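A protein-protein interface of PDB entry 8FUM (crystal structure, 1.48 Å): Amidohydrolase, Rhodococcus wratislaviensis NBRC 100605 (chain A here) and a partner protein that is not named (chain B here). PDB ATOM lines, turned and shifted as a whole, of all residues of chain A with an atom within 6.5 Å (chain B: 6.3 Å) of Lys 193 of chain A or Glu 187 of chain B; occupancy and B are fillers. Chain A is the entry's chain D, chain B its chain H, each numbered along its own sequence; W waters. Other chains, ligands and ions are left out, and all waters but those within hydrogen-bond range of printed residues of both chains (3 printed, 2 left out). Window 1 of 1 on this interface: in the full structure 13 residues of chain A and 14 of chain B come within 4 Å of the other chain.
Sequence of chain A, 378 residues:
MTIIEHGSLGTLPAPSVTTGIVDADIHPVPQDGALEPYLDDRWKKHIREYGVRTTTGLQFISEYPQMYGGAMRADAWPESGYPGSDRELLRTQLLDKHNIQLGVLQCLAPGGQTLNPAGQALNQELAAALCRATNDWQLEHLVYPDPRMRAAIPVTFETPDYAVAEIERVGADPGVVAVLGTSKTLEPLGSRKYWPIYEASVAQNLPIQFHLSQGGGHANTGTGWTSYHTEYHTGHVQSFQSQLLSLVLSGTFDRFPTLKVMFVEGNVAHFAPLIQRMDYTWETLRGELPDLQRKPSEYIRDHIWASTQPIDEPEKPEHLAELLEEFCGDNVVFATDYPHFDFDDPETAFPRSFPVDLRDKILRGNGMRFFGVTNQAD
Water W3 lies within hydrogen-bond range of the side-chain amino group (NZ) of Lys 193 of chain B (2.6 Å), the side-chain carboxylate (OE1) of Glu 158 of chain B (2.8 Å) and the side-chain carboxylate (OE2) of Glu 187 of chain A (3.4 Å).
Water W1 lies within hydrogen-bond range of the side-chain carboxylate of Glu 187 of chain B (3.0 Å) and the backbone carbonyl oxygen of Glu 158 of chain A (3.0 Å).
Water W2 bridges the backbone carbonyl oxygen of Glu 158 of chain B (3.1 Å) and the side-chain carboxylate of Glu 187 of chain A (3.1 Å).
Of the 14 printed residues of chain A, 4 touch a printed residue of chain B.
Hydrophobic or aromatic side chains of chain A within 4 Å of the printed part of chain B: Leu 186.
Of the 16 printed residues of chain B, 4 touch a printed residue of chain A.
Hydrophobic or aromatic side chains of chain B within 4 Å of the printed part of chain A: Leu 186.
Among the printed residues, Asp or Glu carboxylates within 4 Å of a Lys or Arg side-chain nitrogen of the other chain: Glu 187 of chain A with Lys 193 of chain B and Lys 193 of chain A with Glu 187 of chain B.
OE2 of Glu 158 of chain A lies within hydrogen-bond range of N of Leu 186 of chain A (2.8 Å).
NZ of Lys 193 of chain A lies within salt-bridge range of OE1 of Glu 158 of chain A (2.8 Å).
The backbone carbonyl oxygen (O) of Glu 187 of chain B is in hydrogen-bond range of the side-chain hydroxyl (OH) of Tyr 194 of chain B, at 3.3 Å.
OG1 of Thr 185 of chain B lies within hydrogen-bond range of O of Glu 187 of chain B (2.6 Å).
The backbone carbonyl oxygen of Glu 187 of chain A is in hydrogen-bond range of the side-chain hydroxyl of Tyr 194 of chain A (3.3 Å).
OG of Ser 191 of chain B sits at hydrogen-bond distance from OE1 of Glu 187 of chain B, 2.8 Å away.
NZ of Lys 193 of chain B lies within salt-bridge range of OE2 of Glu 187 of chain A, at 3.1 Å.
The side-chain carboxylate (OE2) of Glu 187 of chain B lies within salt-bridge range of the side-chain amino group (NZ) of Lys 193 of chain A (3.2 Å).
CD of Arg 192 of chain B touches CG2 of Thr 159 of chain A, at 3.7 Å.
Leu 186 of chain A touches Leu 186 of chain B (O to CD2, 3.8 Å).
Leu 186 of chain A touches Glu 187 of chain B.
Glu 187 of chain A touches Leu 186 of chain B.
Printed residues of chain B within 4 Å of Thr 159 of chain A: Arg 192.
Glu 187 of chain B touches two residues of chain A.
Of the printed residues of chain A, Lys 193 of chain B touches Glu 187 (3.1 Å).
The nearest residue of chain B that does not touch Lys 193 of chain A is Lys 193 of chain B (5.2 Å).
The nearest residue of chain A that does not touch Glu 187 of chain B is Glu 187 of chain A (4.4 Å).
The nearest printed residue of chain B that does not touch Leu 186 of chain A is His 218 of chain B (4.6 Å).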
ATOM      1  N   PHE A 157      15.967 -15.345  15.142  1.00  0.00           N
ATOM      2  CA  PHE A 157      16.441 -16.515  14.409  1.00  0.00           C
ATOM      3  C   PHE A 157      16.137 -17.805  15.145  1.00  0.00           C
ATOM      4  O   PHE A 157      15.936 -18.837  14.511  1.00  0.00           O
ATOM      5  CB  PHE A 157      17.930 -16.410  14.077  1.00  0.00           C
ATOM      6  CG  PHE A 157      18.172 -15.747  12.759  1.00  0.00           C
ATOM      7  CD1 PHE A 157      18.083 -14.376  12.653  1.00  0.00           C
ATOM      8  CD2 PHE A 157      18.425 -16.493  11.621  1.00  0.00           C
ATOM      9  CE1 PHE A 157      18.262 -13.750  11.428  1.00  0.00           C
ATOM     10  CE2 PHE A 157      18.592 -15.864  10.390  1.00  0.00           C
ATOM     11  CZ  PHE A 157      18.530 -14.506  10.317  1.00  0.00           C
ATOM     12  N   GLU A 158      16.067 -17.775  16.470  1.00  0.00           N
ATOM     13  CA  GLU A 158      15.814 -19.027  17.162  1.00  0.00           C
ATOM     14  C   GLU A 158      14.338 -19.408  17.219  1.00  0.00           C
ATOM     15  O   GLU A 158      14.021 -20.524  17.648  1.00  0.00           O
ATOM     16  CB  GLU A 158      16.436 -19.061  18.552  1.00  0.00           C
ATOM     17  CG  GLU A 158      17.927 -18.809  18.547  1.00  0.00           C
ATOM     18  CD  GLU A 158      18.772 -19.894  17.880  1.00  0.00           C
ATOM     19  OE1 GLU A 158      18.257 -20.779  17.164  1.00  0.00           O
ATOM     20  OE2 GLU A 158      19.995 -19.839  18.115  1.00  0.00           O
ATOM     21  N   THR A 159      13.427 -18.542  16.781  1.00  0.00           N
ATOM     22  CA  THR A 159      12.033 -18.924  16.582  1.00  0.00           C
ATOM     23  C   THR A 159      11.628 -18.498  15.186  1.00  0.00           C
ATOM     24  O   THR A 159      11.067 -17.406  14.998  1.00  0.00           O
ATOM     25  CB  THR A 159      11.113 -18.337  17.649  1.00  0.00           C
ATOM     26  OG1 THR A 159      11.645 -18.633  18.938  1.00  0.00           O
ATOM     27  CG2 THR A 159       9.722 -18.966  17.554  1.00  0.00           C
ATOM     28  N   PRO A 160      11.883 -19.353  14.185  1.00  0.00           N
ATOM     29  CA  PRO A 160      11.628 -18.985  12.781  1.00  0.00           C
ATOM     30  C   PRO A 160      10.216 -18.513  12.497  1.00  0.00           C
ATOM     31  O   PRO A 160      10.062 -17.604  11.685  1.00  0.00           O
ATOM     32  CB  PRO A 160      12.013 -20.264  12.020  1.00  0.00           C
ATOM     33  CG  PRO A 160      13.120 -20.863  12.898  1.00  0.00           C
ATOM     34  CD  PRO A 160      12.654 -20.606  14.300  1.00  0.00           C
ATOM     35  N   LEU A 186      22.172 -21.584  18.361  1.00  0.00           N
ATOM     36  CA  LEU A 186      22.160 -22.866  19.037  1.00  0.00           C
ATOM     37  C   LEU A 186      22.517 -24.009  18.096  1.00  0.00           C
ATOM     38  O   LEU A 186      23.083 -25.026  18.527  1.00  0.00           O
ATOM     39  CB  LEU A 186      20.791 -23.057  19.689  1.00  0.00           C
ATOM     40  CG  LEU A 186      20.693 -24.224  20.686  1.00  0.00           C
ATOM     41  CD1 LEU A 186      21.435 -23.930  21.973  1.00  0.00           C
ATOM     42  CD2 LEU A 186      19.213 -24.523  20.951  1.00  0.00           C
ATOM     43  N   GLU A 187      22.199 -23.859  16.822  1.00  0.00           N
ATOM     44  CA  GLU A 187      22.578 -24.807  15.794  1.00  0.00           C
ATOM     45  C   GLU A 187      23.322 -24.034  14.720  1.00  0.00           C
ATOM     46  O   GLU A 187      23.035 -22.857  14.514  1.00  0.00           O
ATOM     47  CB  GLU A 187      21.328 -25.434  15.146  1.00  0.00           C
ATOM     48  CG  GLU A 187      20.330 -26.022  16.125  1.00  0.00           C
ATOM     49  CD  GLU A 187      19.196 -26.751  15.432  1.00  0.00           C
ATOM     50  OE1 GLU A 187      19.456 -27.366  14.373  1.00  0.00           O
ATOM     51  OE2 GLU A 187      18.079 -26.741  15.974  1.00  0.00           O
ATOM     52  N   GLY A 190      23.561 -23.425   8.801  1.00  0.00           N
ATOM     53  CA  GLY A 190      23.099 -24.249   7.704  1.00  0.00           C
ATOM     54  C   GLY A 190      22.042 -25.251   8.078  1.00  0.00           C
ATOM     55  O   GLY A 190      21.529 -25.956   7.206  1.00  0.00           O
ATOM     56  N   SER A 191      21.696 -25.330   9.358  1.00  0.00           N
ATOM     57  CA  SER A 191      20.666 -26.241   9.820  1.00  0.00           C
ATOM     58  C   SER A 191      19.312 -25.879   9.214  1.00  0.00           C
ATOM     59  O   SER A 191      19.007 -24.702   8.965  1.00  0.00           O
ATOM     60  CB  SER A 191      20.570 -26.164  11.344  1.00  0.00           C
ATOM     61  OG  SER A 191      21.795 -26.522  11.978  1.00  0.00           O
ATOM     62  N   ARG A 192      18.497 -26.913   8.980  1.00  0.00           N
ATOM     63  CA  ARG A 192      17.182 -26.720   8.384  1.00  0.00           C
ATOM     64  C   ARG A 192      16.303 -25.848   9.254  1.00  0.00           C
ATOM     65  O   ARG A 192      15.373 -25.221   8.744  1.00  0.00           O
ATOM     66  CB  ARG A 192      16.525 -28.084   8.131  1.00  0.00           C
ATOM     67  CG  ARG A 192      15.342 -28.012   7.205  1.00  0.00           C
ATOM     68  CD  ARG A 192      14.723 -29.396   7.000  1.00  0.00           C
ATOM     69  NE  ARG A 192      13.575 -29.302   6.107  1.00  0.00           N
ATOM     70  CZ  ARG A 192      13.652 -29.458   4.787  1.00  0.00           C
ATOM     71  NH1 ARG A 192      12.560 -29.352   4.043  1.00  0.00           N
ATOM     72  NH2 ARG A 192      14.810 -29.746   4.215  1.00  0.00           N
ATOM     73  N   LYS A 193      16.618 -25.741  10.544  1.00  0.00           N
ATOM     74  CA  LYS A 193      15.860 -24.872  11.429  1.00  0.00           C
ATOM     75  C   LYS A 193      15.697 -23.481  10.831  1.00  0.00           C
ATOM     76  O   LYS A 193      14.617 -22.895  10.894  1.00  0.00           O
ATOM     77  CB  LYS A 193      16.540 -24.761  12.798  1.00  0.00           C
ATOM     78  CG  LYS A 193      15.905 -23.706  13.689  1.00  0.00           C
ATOM     79  CD  LYS A 193      16.442 -23.685  15.102  1.00  0.00           C
ATOM     80  CE  LYS A 193      15.781 -22.545  15.827  1.00  0.00           C
ATOM     81  NZ  LYS A 193      16.087 -22.487  17.267  1.00  0.00           N
ATOM     82  N   TYR A 194      16.757 -22.947  10.219  1.00  0.00           N
ATOM     83  CA  TYR A 194      16.741 -21.551   9.807  1.00  0.00           C
ATOM     84  C   TYR A 194      16.239 -21.371   8.382  1.00  0.00           C
ATOM     85  O   TYR A 194      16.037 -20.229   7.943  1.00  0.00           O
ATOM     86  CB  TYR A 194      18.142 -20.966   9.975  1.00  0.00           C
ATOM     87  CG  TYR A 194      18.664 -21.163  11.357  1.00  0.00           C
ATOM     88  CD1 TYR A 194      18.053 -20.547  12.440  1.00  0.00           C
ATOM     89  CD2 TYR A 194      19.719 -22.021  11.601  1.00  0.00           C
ATOM     90  CE1 TYR A 194      18.503 -20.754  13.726  1.00  0.00           C
ATOM     91  CE2 TYR A 194      20.186 -22.234  12.908  1.00  0.00           C
ATOM     92  CZ  TYR A 194      19.567 -21.610  13.951  1.00  0.00           C
ATOM     93  OH  TYR A 194      20.009 -21.830  15.251  1.00  0.00           O
ATOM     94  N   TRP A 195      16.001 -22.472   7.675  1.00  0.00           N
ATOM     95  CA  TRP A 195      15.580 -22.382   6.281  1.00  0.00           C
ATOM     96  C   TRP A 195      14.283 -21.600   6.071  1.00  0.00           C
ATOM     97  O   TRP A 195      14.199 -20.857   5.075  1.00  0.00           O
ATOM     98  CB  TRP A 195      15.534 -23.779   5.660  1.00  0.00           C
ATOM     99  CG  TRP A 195      16.891 -24.349   5.371  1.00  0.00           C
ATOM    100  CD1 TRP A 195      18.080 -24.006   5.961  1.00  0.00           C
ATOM    101  CD2 TRP A 195      17.188 -25.362   4.427  1.00  0.00           C
ATOM    102  NE1 TRP A 195      19.107 -24.752   5.425  1.00  0.00           N
ATOM    103  CE2 TRP A 195      18.580 -25.601   4.490  1.00  0.00           C
ATOM    104  CE3 TRP A 195      16.409 -26.105   3.541  1.00  0.00           C
ATOM    105  CZ2 TRP A 195      19.207 -26.538   3.665  1.00  0.00           C
ATOM    106  CZ3 TRP A 195      17.026 -27.043   2.742  1.00  0.00           C
ATOM    107  CH2 TRP A 195      18.407 -27.242   2.796  1.00  0.00           C
ATOM    108  N   PRO A 196      13.282 -21.653   6.950  1.00  0.00           N
ATOM    109  CA  PRO A 196      12.094 -20.799   6.738  1.00  0.00           C
ATOM    110  C   PRO A 196      12.434 -19.326   6.749  1.00  0.00           C
ATOM    111  O   PRO A 196      11.757 -18.544   6.066  1.00  0.00           O
ATOM    112  CB  PRO A 196      11.165 -21.174   7.899  1.00  0.00           C
ATOM    113  CG  PRO A 196      11.581 -22.588   8.229  1.00  0.00           C
ATOM    114  CD  PRO A 196      13.064 -22.646   8.015  1.00  0.00           C
ATOM    115  N   ILE A 197      13.457 -18.918   7.519  1.00  0.00           N
ATOM    116  CA  ILE A 197      13.873 -17.521   7.517  1.00  0.00           C
ATOM    117  C   ILE A 197      14.534 -17.167   6.192  1.00  0.00           C
ATOM    118  O   ILE A 197      14.291 -16.089   5.635  1.00  0.00           O
ATOM    119  CB  ILE A 197      14.784 -17.212   8.724  1.00  0.00           C
ATOM    120  CG1 ILE A 197      14.072 -17.554  10.038  1.00  0.00           C
ATOM    121  CG2 ILE A 197      15.230 -15.753   8.637  1.00  0.00           C
ATOM    122  CD1 ILE A 197      14.961 -17.433  11.251  1.00  0.00           C
ATOM    123  N   GLU B 158      14.700 -33.483  16.185  1.00  0.00           N
ATOM    124  CA  GLU B 158      15.506 -32.307  15.933  1.00  0.00           C
ATOM    125  C   GLU B 158      15.360 -31.779  14.514  1.00  0.00           C
ATOM    126  O   GLU B 158      15.913 -30.714  14.200  1.00  0.00           O
ATOM    127  CB  GLU B 158      16.962 -32.608  16.272  1.00  0.00           C
ATOM    128  CG  GLU B 158      17.141 -33.039  17.712  1.00  0.00           C
ATOM    129  CD  GLU B 158      16.810 -31.967  18.758  1.00  0.00           C
ATOM    130  OE1 GLU B 158      16.188 -30.905  18.480  1.00  0.00           O
ATOM    131  OE2 GLU B 158      17.226 -32.194  19.907  1.00  0.00           O
ATOM    132  N   LYS B 184      16.541 -36.576  26.009  1.00  0.00           N
ATOM    133  CA  LYS B 184      17.431 -35.441  25.839  1.00  0.00           C
ATOM    134  C   LYS B 184      17.278 -34.844  24.446  1.00  0.00           C
ATOM    135  O   LYS B 184      17.180 -35.570  23.446  1.00  0.00           O
ATOM    136  CB  LYS B 184      18.876 -35.846  26.104  1.00  0.00           C
ATOM    137  CG  LYS B 184      19.133 -36.236  27.566  1.00  0.00           C
ATOM    138  CD  LYS B 184      20.587 -36.520  27.838  1.00  0.00           C
ATOM    139  CE  LYS B 184      20.884 -36.785  29.296  1.00  0.00           C
ATOM    140  NZ  LYS B 184      20.124 -37.987  29.749  1.00  0.00           N
ATOM    141  N   THR B 185      17.241 -33.511  24.410  1.00  0.00           N
ATOM    142  CA  THR B 185      17.049 -32.721  23.214  1.00  0.00           C
ATOM    143  C   THR B 185      17.912 -31.472  23.345  1.00  0.00           C
ATOM    144  O   THR B 185      18.420 -31.152  24.427  1.00  0.00           O
ATOM    145  CB  THR B 185      15.576 -32.328  23.059  1.00  0.00           C
ATOM    146  OG1 THR B 185      15.123 -31.726  24.276  1.00  0.00           O
ATOM    147  CG2 THR B 185      14.674 -33.558  22.748  1.00  0.00           C
ATOM    148  N   LEU B 186      18.048 -30.743  22.221  1.00  0.00           N
ATOM    149  CA  LEU B 186      18.886 -29.551  22.185  1.00  0.00           C
ATOM    150  C   LEU B 186      18.164 -28.365  22.795  1.00  0.00           C
ATOM    151  O   LEU B 186      18.799 -27.481  23.365  1.00  0.00           O
ATOM    152  CB  LEU B 186      19.279 -29.252  20.741  1.00  0.00           C
ATOM    153  CG  LEU B 186      20.402 -28.214  20.579  1.00  0.00           C
ATOM    154  CD1 LEU B 186      21.729 -28.791  20.977  1.00  0.00           C
ATOM    155  CD2 LEU B 186      20.463 -27.747  19.102  1.00  0.00           C
ATOM    156  N   GLU B 187      16.838 -28.338  22.688  1.00  0.00           N
ATOM    157  CA  GLU B 187      15.999 -27.377  23.354  1.00  0.00           C
ATOM    158  C   GLU B 187      15.003 -28.124  24.224  1.00  0.00           C
ATOM    159  O   GLU B 187      14.600 -29.239  23.870  1.00  0.00           O
ATOM    160  CB  GLU B 187      15.217 -26.568  22.315  1.00  0.00           C
ATOM    161  CG  GLU B 187      16.108 -25.866  21.316  1.00  0.00           C
ATOM    162  CD  GLU B 187      15.330 -24.949  20.382  1.00  0.00           C
ATOM    163  OE1 GLU B 187      14.504 -24.187  20.900  1.00  0.00           O
ATOM    164  OE2 GLU B 187      15.579 -25.003  19.160  1.00  0.00           O
ATOM    165  N   PRO B 188      14.556 -27.546  25.338  1.00  0.00           N
ATOM    166  CA  PRO B 188      13.550 -28.243  26.153  1.00  0.00           C
ATOM    167  C   PRO B 188      12.268 -28.448  25.346  1.00  0.00           C
ATOM    168  O   PRO B 188      11.925 -27.657  24.468  1.00  0.00           O
ATOM    169  CB  PRO B 188      13.352 -27.320  27.361  1.00  0.00           C
ATOM    170  CG  PRO B 188      14.663 -26.571  27.439  1.00  0.00           C
ATOM    171  CD  PRO B 188      15.085 -26.356  26.029  1.00  0.00           C
ATOM    172  N   LEU B 189      11.570 -29.549  25.643  1.00  0.00           N
ATOM    173  CA  LEU B 189      10.518 -30.037  24.763  1.00  0.00           C
ATOM    174  C   LEU B 189       9.306 -29.116  24.653  1.00  0.00           C
ATOM    175  O   LEU B 189       8.507 -29.295  23.719  1.00  0.00           O
ATOM    176  CB  LEU B 189      10.069 -31.443  25.196  1.00  0.00           C
ATOM    177  CG  LEU B 189      11.000 -32.526  24.681  1.00  0.00           C
ATOM    178  CD1 LEU B 189      10.773 -33.789  25.442  1.00  0.00           C
ATOM    179  CD2 LEU B 189      10.834 -32.757  23.186  1.00  0.00           C
ATOM    180  N   GLY B 190       9.134 -28.160  25.560  1.00  0.00           N
ATOM    181  CA  GLY B 190       8.091 -27.155  25.393  1.00  0.00           C
ATOM    182  C   GLY B 190       8.382 -26.097  24.345  1.00  0.00           C
ATOM    183  O   GLY B 190       7.491 -25.295  24.034  1.00  0.00           O
ATOM    184  N   SER B 191       9.582 -26.100  23.784  1.00  0.00           N
ATOM    185  CA  SER B 191       9.973 -25.123  22.772  1.00  0.00           C
ATOM    186  C   SER B 191       9.093 -25.228  21.538  1.00  0.00           C
ATOM    187  O   SER B 191       8.711 -26.319  21.110  1.00  0.00           O
ATOM    188  CB  SER B 191      11.404 -25.391  22.322  1.00  0.00           C
ATOM    189  OG  SER B 191      11.708 -24.636  21.151  1.00  0.00           O
ATOM    190  N   ARG B 192       8.827 -24.078  20.924  1.00  0.00           N
ATOM    191  CA  ARG B 192       8.015 -24.060  19.709  1.00  0.00           C
ATOM    192  C   ARG B 192       8.641 -24.890  18.592  1.00  0.00           C
ATOM    193  O   ARG B 192       7.927 -25.318  17.683  1.00  0.00           O
ATOM    194  CB  ARG B 192       7.814 -22.600  19.267  1.00  0.00           C
ATOM    195  CG  ARG B 192       6.788 -22.410  18.159  1.00  0.00           C
ATOM    196  CD  ARG B 192       6.609 -20.945  17.780  1.00  0.00           C
ATOM    197  NE  ARG B 192       5.606 -20.810  16.726  1.00  0.00           N
ATOM    198  CZ  ARG B 192       4.319 -20.555  16.948  1.00  0.00           C
ATOM    199  NH1 ARG B 192       3.859 -20.407  18.182  1.00  0.00           N
ATOM    200  NH2 ARG B 192       3.488 -20.448  15.922  1.00  0.00           N
ATOM    201  N   LYS B 193       9.944 -25.160  18.647  1.00  0.00           N
ATOM    202  CA  LYS B 193      10.557 -26.010  17.629  1.00  0.00           C
ATOM    203  C   LYS B 193       9.778 -27.303  17.431  1.00  0.00           C
ATOM    204  O   LYS B 193       9.598 -27.769  16.300  1.00  0.00           O
ATOM    205  CB  LYS B 193      11.988 -26.353  18.037  1.00  0.00           C
ATOM    206  CG  LYS B 193      12.625 -27.409  17.154  1.00  0.00           C
ATOM    207  CD  LYS B 193      14.075 -27.664  17.461  1.00  0.00           C
ATOM    208  CE  LYS B 193      14.600 -28.656  16.443  1.00  0.00           C
ATOM    209  NZ  LYS B 193      16.049 -28.979  16.559  1.00  0.00           N
ATOM    210  N   TYR B 194       9.348 -27.923  18.531  1.00  0.00           N
ATOM    211  CA  TYR B 194       8.734 -29.244  18.493  1.00  0.00           C
ATOM    212  C   TYR B 194       7.232 -29.206  18.236  1.00  0.00           C
ATOM    213  O   TYR B 194       6.639 -30.258  17.979  1.00  0.00           O
ATOM    214  CB  TYR B 194       9.070 -30.029  19.772  1.00  0.00           C
ATOM    215  CG  TYR B 194      10.557 -30.046  20.024  1.00  0.00           C
ATOM    216  CD1 TYR B 194      11.415 -30.728  19.183  1.00  0.00           C
ATOM    217  CD2 TYR B 194      11.109 -29.317  21.069  1.00  0.00           C
ATOM    218  CE1 TYR B 194      12.814 -30.702  19.380  1.00  0.00           C
ATOM    219  CE2 TYR B 194      12.484 -29.289  21.274  1.00  0.00           C
ATOM    220  CZ  TYR B 194      13.330 -29.971  20.424  1.00  0.00           C
ATOM    221  OH  TYR B 194      14.693 -29.915  20.650  1.00  0.00           O
ATOM    222  N   GLY B 216      21.715 -35.575  22.907  1.00  0.00           N
ATOM    223  CA  GLY B 216      20.876 -34.408  22.966  1.00  0.00           C
ATOM    224  C   GLY B 216      21.587 -33.113  22.593  1.00  0.00           C
ATOM    225  O   GLY B 216      20.923 -32.176  22.120  1.00  0.00           O
ATOM    226  N   HIS B 218      23.780 -31.452  24.893  1.00  0.00           N
ATOM    227  CA  HIS B 218      24.296 -30.903  26.143  1.00  0.00           C
ATOM    228  C   HIS B 218      24.893 -32.022  26.984  1.00  0.00           C
ATOM    229  O   HIS B 218      24.703 -33.209  26.719  1.00  0.00           O
ATOM    230  CB  HIS B 218      23.178 -30.186  26.920  1.00  0.00           C
ATOM    231  CG  HIS B 218      22.482 -29.156  26.107  1.00  0.00           C
ATOM    232  ND1 HIS B 218      23.029 -27.909  25.872  1.00  0.00           N
ATOM    233  CD2 HIS B 218      21.349 -29.225  25.371  1.00  0.00           C
ATOM    234  CE1 HIS B 218      22.223 -27.237  25.068  1.00  0.00           C
ATOM    235  NE2 HIS B 218      21.210 -28.019  24.741  1.00  0.00           N
ATOM    236  N   GLN B 243      12.320 -31.781  31.263  1.00  0.00           N
ATOM    237  CA  GLN B 243      11.349 -31.831  30.168  1.00  0.00           C
ATOM    238  C   GLN B 243       9.936 -31.606  30.682  1.00  0.00           C
ATOM    239  O   GLN B 243       9.136 -30.909  30.052  1.00  0.00           O
ATOM    240  CB  GLN B 243      11.437 -33.170  29.422  1.00  0.00           C
ATOM    241  CG  GLN B 243      12.768 -33.455  28.732  1.00  0.00           C
ATOM    242  CD  GLN B 243      13.052 -32.544  27.543  1.00  0.00           C
ATOM    243  OE1 GLN B 243      12.518 -31.422  27.435  1.00  0.00           O
ATOM    244  NE2 GLN B 243      13.927 -33.006  26.666  1.00  0.00           N
ATOM    245  N   SER B 246       9.383 -27.870  31.244  1.00  0.00           N
ATOM    246  CA  SER B 246       9.249 -27.099  30.012  1.00  0.00           C
ATOM    247  C   SER B 246       7.907 -27.367  29.347  1.00  0.00           C
ATOM    248  O   SER B 246       7.188 -26.429  28.949  1.00  0.00           O
ATOM    249  CB  SER B 246      10.403 -27.426  29.069  1.00  0.00           C
ATOM    250  OG  SER B 246      10.195 -26.899  27.763  1.00  0.00           O
HETATM  251  O   HOH W   1      14.555 -21.194  20.566  1.00  0.00           O
HETATM  252  O   HOH W   2      18.996 -30.427  14.153  1.00  0.00           O
HETATM  253  O   HOH W   3      18.463 -29.905  17.089  1.00  0.00           O
